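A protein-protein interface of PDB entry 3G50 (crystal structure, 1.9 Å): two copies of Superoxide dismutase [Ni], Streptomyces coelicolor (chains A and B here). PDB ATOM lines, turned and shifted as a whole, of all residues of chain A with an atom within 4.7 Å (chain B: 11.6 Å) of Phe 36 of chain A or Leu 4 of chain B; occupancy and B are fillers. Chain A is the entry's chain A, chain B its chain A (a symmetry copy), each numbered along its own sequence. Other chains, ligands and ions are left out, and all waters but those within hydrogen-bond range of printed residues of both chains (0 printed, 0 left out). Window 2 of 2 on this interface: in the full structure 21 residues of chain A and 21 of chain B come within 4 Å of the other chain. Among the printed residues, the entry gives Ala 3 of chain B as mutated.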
ATOM      1  N   VAL A  24       9.362  15.351  24.716  1.00  0.00           N
ATOM      2  CA  VAL A  24      10.260  15.444  23.567  1.00  0.00           C
ATOM      3  C   VAL A  24      10.888  16.855  23.488  1.00  0.00           C
ATOM      4  O   VAL A  24      12.116  17.013  23.297  1.00  0.00           O
ATOM      5  CB  VAL A  24       9.558  15.104  22.256  1.00  0.00           C
ATOM      6  CG1 VAL A  24      10.407  15.554  21.083  1.00  0.00           C
ATOM      7  CG2 VAL A  24       9.222  13.582  22.215  1.00  0.00           C
ATOM      8  N   LYS A  27      13.668  17.061  25.922  1.00  0.00           N
ATOM      9  CA  LYS A  27      14.853  16.311  25.466  1.00  0.00           C
ATOM     10  C   LYS A  27      15.623  17.032  24.358  1.00  0.00           C
ATOM     11  O   LYS A  27      16.862  16.951  24.290  1.00  0.00           O
ATOM     12  CB  LYS A  27      14.520  14.855  25.097  1.00  0.00           C
ATOM     13  CG  LYS A  27      14.390  14.005  26.333  1.00  0.00           C
ATOM     14  CD  LYS A  27      13.800  12.639  26.071  1.00  0.00           C
ATOM     15  CE  LYS A  27      13.310  11.989  27.394  1.00  0.00           C
ATOM     16  NZ  LYS A  27      14.261  12.013  28.585  1.00  0.00           N
ATOM     17  N   MET A  28      14.919  17.772  23.509  1.00  0.00           N
ATOM     18  CA  MET A  28      15.607  18.549  22.463  1.00  0.00           C
ATOM     19  C   MET A  28      16.558  19.645  23.005  1.00  0.00           C
ATOM     20  O   MET A  28      17.494  20.046  22.319  1.00  0.00           O
ATOM     21  CB  MET A  28      14.600  19.165  21.506  1.00  0.00           C
ATOM     22  CG  MET A  28      13.703  18.101  20.811  1.00  0.00           C
ATOM     23  SD  MET A  28      12.542  18.909  19.725  1.00  0.00           S
ATOM     24  CE  MET A  28      13.533  19.204  18.257  1.00  0.00           C
ATOM     25  N   ASN A  31      20.369  17.720  23.933  1.00  0.00           N
ATOM     26  CA  ASN A  31      21.158  16.925  22.981  1.00  0.00           C
ATOM     27  C   ASN A  31      21.166  17.547  21.595  1.00  0.00           C
ATOM     28  O   ASN A  31      20.202  17.382  20.831  1.00  0.00           O
ATOM     29  CB  ASN A  31      20.597  15.486  22.928  1.00  0.00           C
ATOM     30  CG  ASN A  31      21.368  14.560  21.975  1.00  0.00           C
ATOM     31  OD1 ASN A  31      22.338  14.966  21.292  1.00  0.00           O
ATOM     32  ND2 ASN A  31      20.929  13.293  21.925  1.00  0.00           N
ATOM     33  N   ASP A  33      22.694  16.817  18.904  1.00  0.00           N
ATOM     34  CA  ASP A  33      22.898  15.915  17.771  1.00  0.00           C
ATOM     35  C   ASP A  33      21.798  16.140  16.720  1.00  0.00           C
ATOM     36  O   ASP A  33      20.609  16.011  17.031  1.00  0.00           O
ATOM     37  CB  ASP A  33      22.931  14.449  18.229  1.00  0.00           C
ATOM     38  CG  ASP A  33      23.064  13.487  17.051  1.00  0.00           C
ATOM     39  OD1 ASP A  33      22.336  12.462  16.979  1.00  0.00           O
ATOM     40  OD2 ASP A  33      23.882  13.783  16.162  1.00  0.00           O
ATOM     41  N   PRO A  34      22.181  16.545  15.496  1.00  0.00           N
ATOM     42  CA  PRO A  34      21.236  16.866  14.423  1.00  0.00           C
ATOM     43  C   PRO A  34      20.306  15.675  14.062  1.00  0.00           C
ATOM     44  O   PRO A  34      19.137  15.861  13.796  1.00  0.00           O
ATOM     45  CB  PRO A  34      22.150  17.205  13.235  1.00  0.00           C
ATOM     46  CG  PRO A  34      23.434  17.533  13.812  1.00  0.00           C
ATOM     47  CD  PRO A  34      23.581  16.755  15.082  1.00  0.00           C
ATOM     48  N   HIS A  35      20.847  14.465  14.073  1.00  0.00           N
ATOM     49  CA  HIS A  35      20.038  13.278  13.843  1.00  0.00           C
ATOM     50  C   HIS A  35      18.998  13.081  14.940  1.00  0.00           C
ATOM     51  O   HIS A  35      17.833  12.873  14.640  1.00  0.00           O
ATOM     52  CB  HIS A  35      20.912  12.048  13.700  1.00  0.00           C
ATOM     53  CG  HIS A  35      20.143  10.815  13.372  1.00  0.00           C
ATOM     54  ND1 HIS A  35      20.189   9.692  14.158  1.00  0.00           N
ATOM     55  CD2 HIS A  35      19.284  10.535  12.360  1.00  0.00           C
ATOM     56  CE1 HIS A  35      19.426   8.755  13.629  1.00  0.00           C
ATOM     57  NE2 HIS A  35      18.862   9.242  12.542  1.00  0.00           N
ATOM     58  N   PHE A  36      19.418  13.171  16.199  1.00  0.00           N
ATOM     59  CA  PHE A  36      18.494  13.157  17.339  1.00  0.00           C
ATOM     60  C   PHE A  36      17.480  14.311  17.237  1.00  0.00           C
ATOM     61  O   PHE A  36      16.281  14.109  17.415  1.00  0.00           O
ATOM     62  CB  PHE A  36      19.245  13.190  18.684  1.00  0.00           C
ATOM     63  CG  PHE A  36      18.345  13.303  19.870  1.00  0.00           C
ATOM     64  CD1 PHE A  36      17.963  14.557  20.356  1.00  0.00           C
ATOM     65  CD2 PHE A  36      17.834  12.166  20.472  1.00  0.00           C
ATOM     66  CE1 PHE A  36      17.089  14.673  21.449  1.00  0.00           C
ATOM     67  CE2 PHE A  36      16.940  12.275  21.557  1.00  0.00           C
ATOM     68  CZ  PHE A  36      16.572  13.538  22.039  1.00  0.00           C
ATOM     69  N   GLN A  37      17.935  15.510  16.884  1.00  0.00           N
ATOM     70  CA  GLN A  37      16.997  16.647  16.728  1.00  0.00           C
ATOM     71  C   GLN A  37      15.912  16.362  15.700  1.00  0.00           C
ATOM     72  O   GLN A  37      14.728  16.719  15.892  1.00  0.00           O
ATOM     73  CB  GLN A  37      17.742  17.908  16.284  1.00  0.00           C
ATOM     74  CG  GLN A  37      18.649  18.449  17.359  1.00  0.00           C
ATOM     75  CD  GLN A  37      17.880  19.163  18.475  1.00  0.00           C
ATOM     76  OE1 GLN A  37      16.998  19.989  18.221  1.00  0.00           O
ATOM     77  NE2 GLN A  37      18.224  18.846  19.718  1.00  0.00           N
ATOM     78  N   THR A  38      16.316  15.753  14.593  1.00  0.00           N
ATOM     79  CA  THR A  38      15.364  15.397  13.539  1.00  0.00           C
ATOM     80  C   THR A  38      14.401  14.304  14.004  1.00  0.00           C
ATOM     81  O   THR A  38      13.221  14.415  13.788  1.00  0.00           O
ATOM     82  CB  THR A  38      16.121  14.936  12.289  1.00  0.00           C
ATOM     83  OG1 THR A  38      16.901  16.029  11.786  1.00  0.00           O
ATOM     84  CG2 THR A  38      15.184  14.413  11.226  1.00  0.00           C
ATOM     85  N   ARG A  39      14.915  13.224  14.596  1.00  0.00           N
ATOM     86  CA  ARG A  39      14.010  12.174  15.117  1.00  0.00           C
ATOM     87  C   ARG A  39      12.993  12.780  16.121  1.00  0.00           C
ATOM     88  O   ARG A  39      11.775  12.510  16.056  1.00  0.00           O
ATOM     89  CB  ARG A  39      14.791  11.001  15.768  1.00  0.00           C
ATOM     90  CG  ARG A  39      15.670  10.231  14.820  1.00  0.00           C
ATOM     91  CD  ARG A  39      16.296   8.956  15.478  1.00  0.00           C
ATOM     92  NE  ARG A  39      15.228   8.187  16.099  1.00  0.00           N
ATOM     93  CZ  ARG A  39      15.061   7.964  17.400  1.00  0.00           C
ATOM     94  NH1 ARG A  39      15.971   8.370  18.331  1.00  0.00           N
ATOM     95  NH2 ARG A  39      13.965   7.316  17.751  1.00  0.00           N
ATOM     96  N   ALA A  40      13.488  13.557  17.093  1.00  0.00           N
ATOM     97  CA  ALA A  40      12.624  14.262  18.050  1.00  0.00           C
ATOM     98  C   ALA A  40      11.543  15.053  17.320  1.00  0.00           C
ATOM     99  O   ALA A  40      10.377  15.044  17.735  1.00  0.00           O
ATOM    100  CB  ALA A  40      13.456  15.227  18.936  1.00  0.00           C
ATOM    101  N   ILE A  43       8.905  12.590  15.822  1.00  0.00           N
ATOM    102  CA  ILE A  43       8.055  12.069  16.898  1.00  0.00           C
ATOM    103  C   ILE A  43       7.087  13.131  17.384  1.00  0.00           C
ATOM    104  O   ILE A  43       5.883  12.895  17.527  1.00  0.00           O
ATOM    105  CB  ILE A  43       8.918  11.467  18.038  1.00  0.00           C
ATOM    106  CG1 ILE A  43       9.642  10.241  17.473  1.00  0.00           C
ATOM    107  CG2 ILE A  43       8.042  11.095  19.307  1.00  0.00           C
ATOM    108  CD1 ILE A  43      10.828   9.806  18.238  1.00  0.00           C
ATOM    109  N   HIS B   1       6.543   6.103  24.541  1.00  0.00           N
ATOM    110  CA  HIS B   1       5.813   5.150  23.652  1.00  0.00           C
ATOM    111  C   HIS B   1       6.165   5.352  22.164  1.00  0.00           C
ATOM    112  O   HIS B   1       5.401   4.969  21.269  1.00  0.00           O
ATOM    113  CB  HIS B   1       4.300   5.230  23.915  1.00  0.00           C
ATOM    114  CG  HIS B   1       3.763   6.627  23.981  1.00  0.00           C
ATOM    115  ND1 HIS B   1       3.932   7.543  22.960  1.00  0.00           N
ATOM    116  CD2 HIS B   1       3.043   7.259  24.937  1.00  0.00           C
ATOM    117  CE1 HIS B   1       3.339   8.675  23.287  1.00  0.00           C
ATOM    118  NE2 HIS B   1       2.797   8.533  24.484  1.00  0.00           N
ATOM    119  N   CYS B   2       7.347   5.928  21.930  1.00  0.00           N
ATOM    120  CA  CYS B   2       7.807   6.354  20.596  1.00  0.00           C
ATOM    121  C   CYS B   2       9.264   5.942  20.313  1.00  0.00           C
ATOM    122  O   CYS B   2       9.732   6.073  19.176  1.00  0.00           O
ATOM    123  CB  CYS B   2       7.660   7.877  20.453  1.00  0.00           C
ATOM    124  SG  CYS B   2       8.729   8.852  21.604  1.00  0.00           S
ATOM    125  N   ALA B   3       9.955   5.454  21.355  1.00  0.00           N
ATOM    126  CA  ALA B   3      11.371   5.004  21.310  1.00  0.00           C
ATOM    127  C   ALA B   3      12.406   6.063  20.871  1.00  0.00           C
ATOM    128  O   ALA B   3      13.480   5.718  20.358  1.00  0.00           O
ATOM    129  CB  ALA B   3      11.536   3.655  20.522  1.00  0.00           C
ATOM    130  N   LEU B   4      12.079   7.341  21.095  1.00  0.00           N
ATOM    131  CA  LEU B   4      13.030   8.477  20.932  1.00  0.00           C
ATOM    132  C   LEU B   4      14.387   8.316  21.679  1.00  0.00           C
ATOM    133  O   LEU B   4      15.445   8.502  21.064  1.00  0.00           O
ATOM    134  CB  LEU B   4      12.358   9.826  21.284  1.00  0.00           C
ATOM    135  CG  LEU B   4      13.231  11.086  21.398  1.00  0.00           C
ATOM    136  CD1 LEU B   4      13.924  11.450  20.087  1.00  0.00           C
ATOM    137  CD2 LEU B   4      12.386  12.227  21.879  1.00  0.00           C
ATOM    138  N   PRO B   5      14.362   7.962  22.995  1.00  0.00           N
ATOM    139  CA  PRO B   5      13.179   7.710  23.830  1.00  0.00           C
ATOM    140  C   PRO B   5      12.674   8.993  24.495  1.00  0.00           C
ATOM    141  O   PRO B   5      13.461   9.893  24.817  1.00  0.00           O
ATOM    142  CB  PRO B   5      13.681   6.694  24.875  1.00  0.00           C
ATOM    143  CG  PRO B   5      15.200   6.875  24.930  1.00  0.00           C
ATOM    144  CD  PRO B   5      15.617   7.763  23.754  1.00  0.00           C
ATOM    145  N   CYS B   6      11.365   9.077  24.673  1.00  0.00           N
ATOM    146  CA  CYS B   6      10.780  10.215  25.346  1.00  0.00           C
ATOM    147  C   CYS B   6      10.488   9.893  26.827  1.00  0.00           C
ATOM    148  O   CYS B   6      10.253  10.813  27.625  1.00  0.00           O
ATOM    149  CB  CYS B   6       9.516  10.668  24.605  1.00  0.00           C
ATOM    150  SG  CYS B   6       8.006   9.727  25.004  1.00  0.00           S
ATOM    151  N   GLY B   7      10.510   8.598  27.186  1.00  0.00           N
ATOM    152  CA  GLY B   7      10.161   8.132  28.555  1.00  0.00           C
ATOM    153  C   GLY B   7       8.730   8.386  29.074  1.00  0.00           C
ATOM    154  O   GLY B   7       8.527   8.425  30.297  1.00  0.00           O
ATOM    155  N   VAL B   8       7.741   8.580  28.181  1.00  0.00           N
ATOM    156  CA  VAL B   8       6.305   8.672  28.595  1.00  0.00           C
ATOM    157  C   VAL B   8       5.511   7.379  28.245  1.00  0.00           C
ATOM    158  O   VAL B   8       5.037   7.190  27.126  1.00  0.00           O
ATOM    159  CB  VAL B   8       5.567   9.918  28.025  1.00  0.00           C
ATOM    160  CG1 VAL B   8       4.075   9.925  28.450  1.00  0.00           C
ATOM    161  CG2 VAL B   8       6.233  11.213  28.474  1.00  0.00           C
ATOM    162  N   TYR B   9       5.390   6.493  29.220  1.00  0.00           N
ATOM    163  CA  TYR B   9       4.669   5.249  29.053  1.00  0.00           C
ATOM    164  C   TYR B   9       3.583   5.194  30.094  1.00  0.00           C
ATOM    165  O   TYR B   9       3.729   5.750  31.185  1.00  0.00           O
ATOM    166  CB  TYR B   9       5.619   4.043  29.157  1.00  0.00           C
ATOM    167  CG  TYR B   9       6.591   4.015  27.999  1.00  0.00           C
ATOM    168  CD1 TYR B   9       7.874   4.593  28.114  1.00  0.00           C
ATOM    169  CD2 TYR B   9       6.207   3.493  26.762  1.00  0.00           C
ATOM    170  CE1 TYR B   9       8.749   4.616  27.035  1.00  0.00           C
ATOM    171  CE2 TYR B   9       7.083   3.506  25.675  1.00  0.00           C
ATOM    172  CZ  TYR B   9       8.341   4.065  25.814  1.00  0.00           C
ATOM    173  OH  TYR B   9       9.176   4.060  24.723  1.00  0.00           O
ATOM    174  N   VAL B  57       4.528  -2.213  22.790  1.00  0.00           N
ATOM    175  CA  VAL B  57       5.396  -1.063  23.031  1.00  0.00           C
ATOM    176  C   VAL B  57       5.938  -1.014  24.464  1.00  0.00           C
ATOM    177  O   VAL B  57       7.119  -0.704  24.668  1.00  0.00           O
ATOM    178  CB  VAL B  57       4.668   0.238  22.638  1.00  0.00           C
ATOM    179  CG1 VAL B  57       5.377   1.463  23.237  1.00  0.00           C
ATOM    180  CG2 VAL B  57       4.697   0.340  21.111  1.00  0.00           C
ATOM    181  N   SER B  60       8.551  -3.710  24.642  1.00  0.00           N
ATOM    182  CA  SER B  60       9.785  -3.568  23.903  1.00  0.00           C
ATOM    183  C   SER B  60      10.552  -2.308  24.285  1.00  0.00           C
ATOM    184  O   SER B  60      11.805  -2.296  24.373  1.00  0.00           O
ATOM    185  CB  SER B  60       9.491  -3.580  22.423  1.00  0.00           C
ATOM    186  OG  SER B  60       8.754  -2.451  22.062  1.00  0.00           O
ATOM    187  N   ASP B  61       9.804  -1.250  24.533  1.00  0.00           N
ATOM    188  CA  ASP B  61      10.389   0.060  24.648  1.00  0.00           C
ATOM    189  C   ASP B  61      10.403   0.557  26.104  1.00  0.00           C
ATOM    190  O   ASP B  61      11.139   1.489  26.410  1.00  0.00           O
ATOM    191  CB  ASP B  61       9.629   1.099  23.812  1.00  0.00           C
ATOM    192  CG  ASP B  61       9.694   0.833  22.298  1.00  0.00           C
ATOM    193  OD1 ASP B  61      10.215  -0.190  21.817  1.00  0.00           O
ATOM    194  OD2 ASP B  61       9.160   1.684  21.594  1.00  0.00           O
ATOM    195  N   TYR B  62       9.575   0.003  26.998  1.00  0.00           N
ATOM    196  CA  TYR B  62       9.604   0.532  28.370  1.00  0.00           C
ATOM    197  C   TYR B  62      10.375  -0.439  29.288  1.00  0.00           C
ATOM    198  O   TYR B  62      11.393  -0.055  29.914  1.00  0.00           O
ATOM    199  CB  TYR B  62       8.220   0.910  28.942  1.00  0.00           C
ATOM    200  CG  TYR B  62       8.338   1.227  30.427  1.00  0.00           C
ATOM    201  CD1 TYR B  62       8.770   2.492  30.867  1.00  0.00           C
ATOM    202  CD2 TYR B  62       8.121   0.249  31.367  1.00  0.00           C
ATOM    203  CE1 TYR B  62       8.930   2.766  32.231  1.00  0.00           C
ATOM    204  CE2 TYR B  62       8.264   0.492  32.725  1.00  0.00           C
ATOM    205  CZ  TYR B  62       8.689   1.771  33.156  1.00  0.00           C
ATOM    206  OH  TYR B  62       8.835   2.036  34.505  1.00  0.00           O
ATOM    207  N   LYS B  64      12.909  -3.097  30.702  1.00  0.00           N
ATOM    208  CA  LYS B  64      14.350  -3.285  30.484  1.00  0.00           C
ATOM    209  C   LYS B  64      14.881  -4.539  31.176  1.00  0.00           C
ATOM    210  O   LYS B  64      14.173  -5.143  31.979  1.00  0.00           O
ATOM    211  CB  LYS B  64      15.085  -2.031  30.917  1.00  0.00           C
ATOM    212  CG  LYS B  64      14.640  -0.845  30.078  1.00  0.00           C
ATOM    213  CD  LYS B  64      15.430   0.398  30.349  1.00  0.00           C
ATOM    214  CE  LYS B  64      15.596   1.195  29.058  1.00  0.00           C
ATOM    215  NZ  LYS B  64      14.296   1.475  28.396  1.00  0.00           N
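Among the printed residues, pairs that only touch across the chains: Val 24 of chain A with Leu 4 of chain B (3.5 Å), Val 24 of chain A with Cys 6 of chain B (3.8 Å), Lys 27 of chain A with Pro 5 of chain B (3.0 Å), Lys 27 of chain A with Cys 6 of chain B (3.3 Å), Phe 36 of chain A with Leu 4 of chain B (3.5 Å), Ala 40 of chain A with Leu 4 of chain B (3.7 Å), Ile 43 of chain A with Cys 2 of chain B (3.3 Å) and Ile 43 of chain A with Leu 4 of chain B (3.4 Å).
Printed residues of chain A that touch a printed residue of chain B: Val 24, Lys 27, Phe 36, Arg 39, Ala 40 and Ile 43.
Among the printed residues, no Asp or Glu carboxylate lies within 4 Å of a Lys or Arg side-chain nitrogen of the other chain.
No position is printed for both chains.
Of the 10 pairs that touch across the chains among the printed residues, none has its exchanged pair printed and touching as well.
The side-chain sulfur (SG) of Cys 2 of chain B sits close to the backbone NH (N) of Leu 4 of chain B (3.7 Å).
The backbone NH (N) of Val 8 of chain B sits close to the side-chain sulfur (SG) of Cys 6 of chain B (3.4 Å).
OD1 of Asp 33 of chain A sits at hydrogen-bond distance from N of Phe 36 of chain A (3.1 Å).
Lys 27 of chain A touches two residues of chain B.
No residue of chain B comes within 4 Å of Met 28 of chain A.
No residue of chain B comes within 4 Å of Asn 31 of chain A.
No residue of chain B comes within 4 Å of Asp 33 of chain A.
Pro 34 of chain A touches none of the printed residues of chain B.
No residue of chain B comes within 4 Å of His 35 of chain A.
Phe 36 of chain A touches one residue of chain B.
Arg 39 of chain A touches just these residues of chain B: Ala 3 (3.1 Å) and Leu 4 (2.8 Å).
Ala 40 of chain A touches just one residue of chain B: Leu 4 (3.7 Å).
Printed residues of chain B within 4 Å of Ile 43 of chain A: Cys 2 and Leu 4.
Of the printed residues of chain A, Cys 2 of chain B touches Ile 43.
Printed residues of chain A within 4 Å of Ala 3 of chain B: Arg 39 (3.1 Å).
Leu 4 of chain B touches just these residues of chain A: Val 24 (3.5 Å), Phe 36 (3.5 Å), Arg 39 (2.8 Å), Ala 40 (3.7 Å) and Ile 43 (3.4 Å).
Of the printed residues of chain A, Pro 5 of chain B touches Lys 27 (3.0 Å).
Of the printed residues of chain A, Cys 6 of chain B touches Val 24 (3.8 Å) and Lys 27 (3.3 Å).
Tyr 9 of chain B touches none of the printed residues of chain A.
Tyr 62 of chain B touches none of the printed residues of chain A.
The nearest residue of chain B that does not touch Phe 36 of chain A is Pro 5 of chain B (5.2 Å).
The nearest residue of chain A that does not touch Leu 4 of chain B is Lys 27 of chain A (4.4 Å).
NH1 of Arg 39 of chain A sits at hydrogen-bond distance from O of Leu 4 of chain B.
NH2 of Arg 39 of chain A lies within hydrogen-bond range of O of Ala 3 of chain B (3.1 Å).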
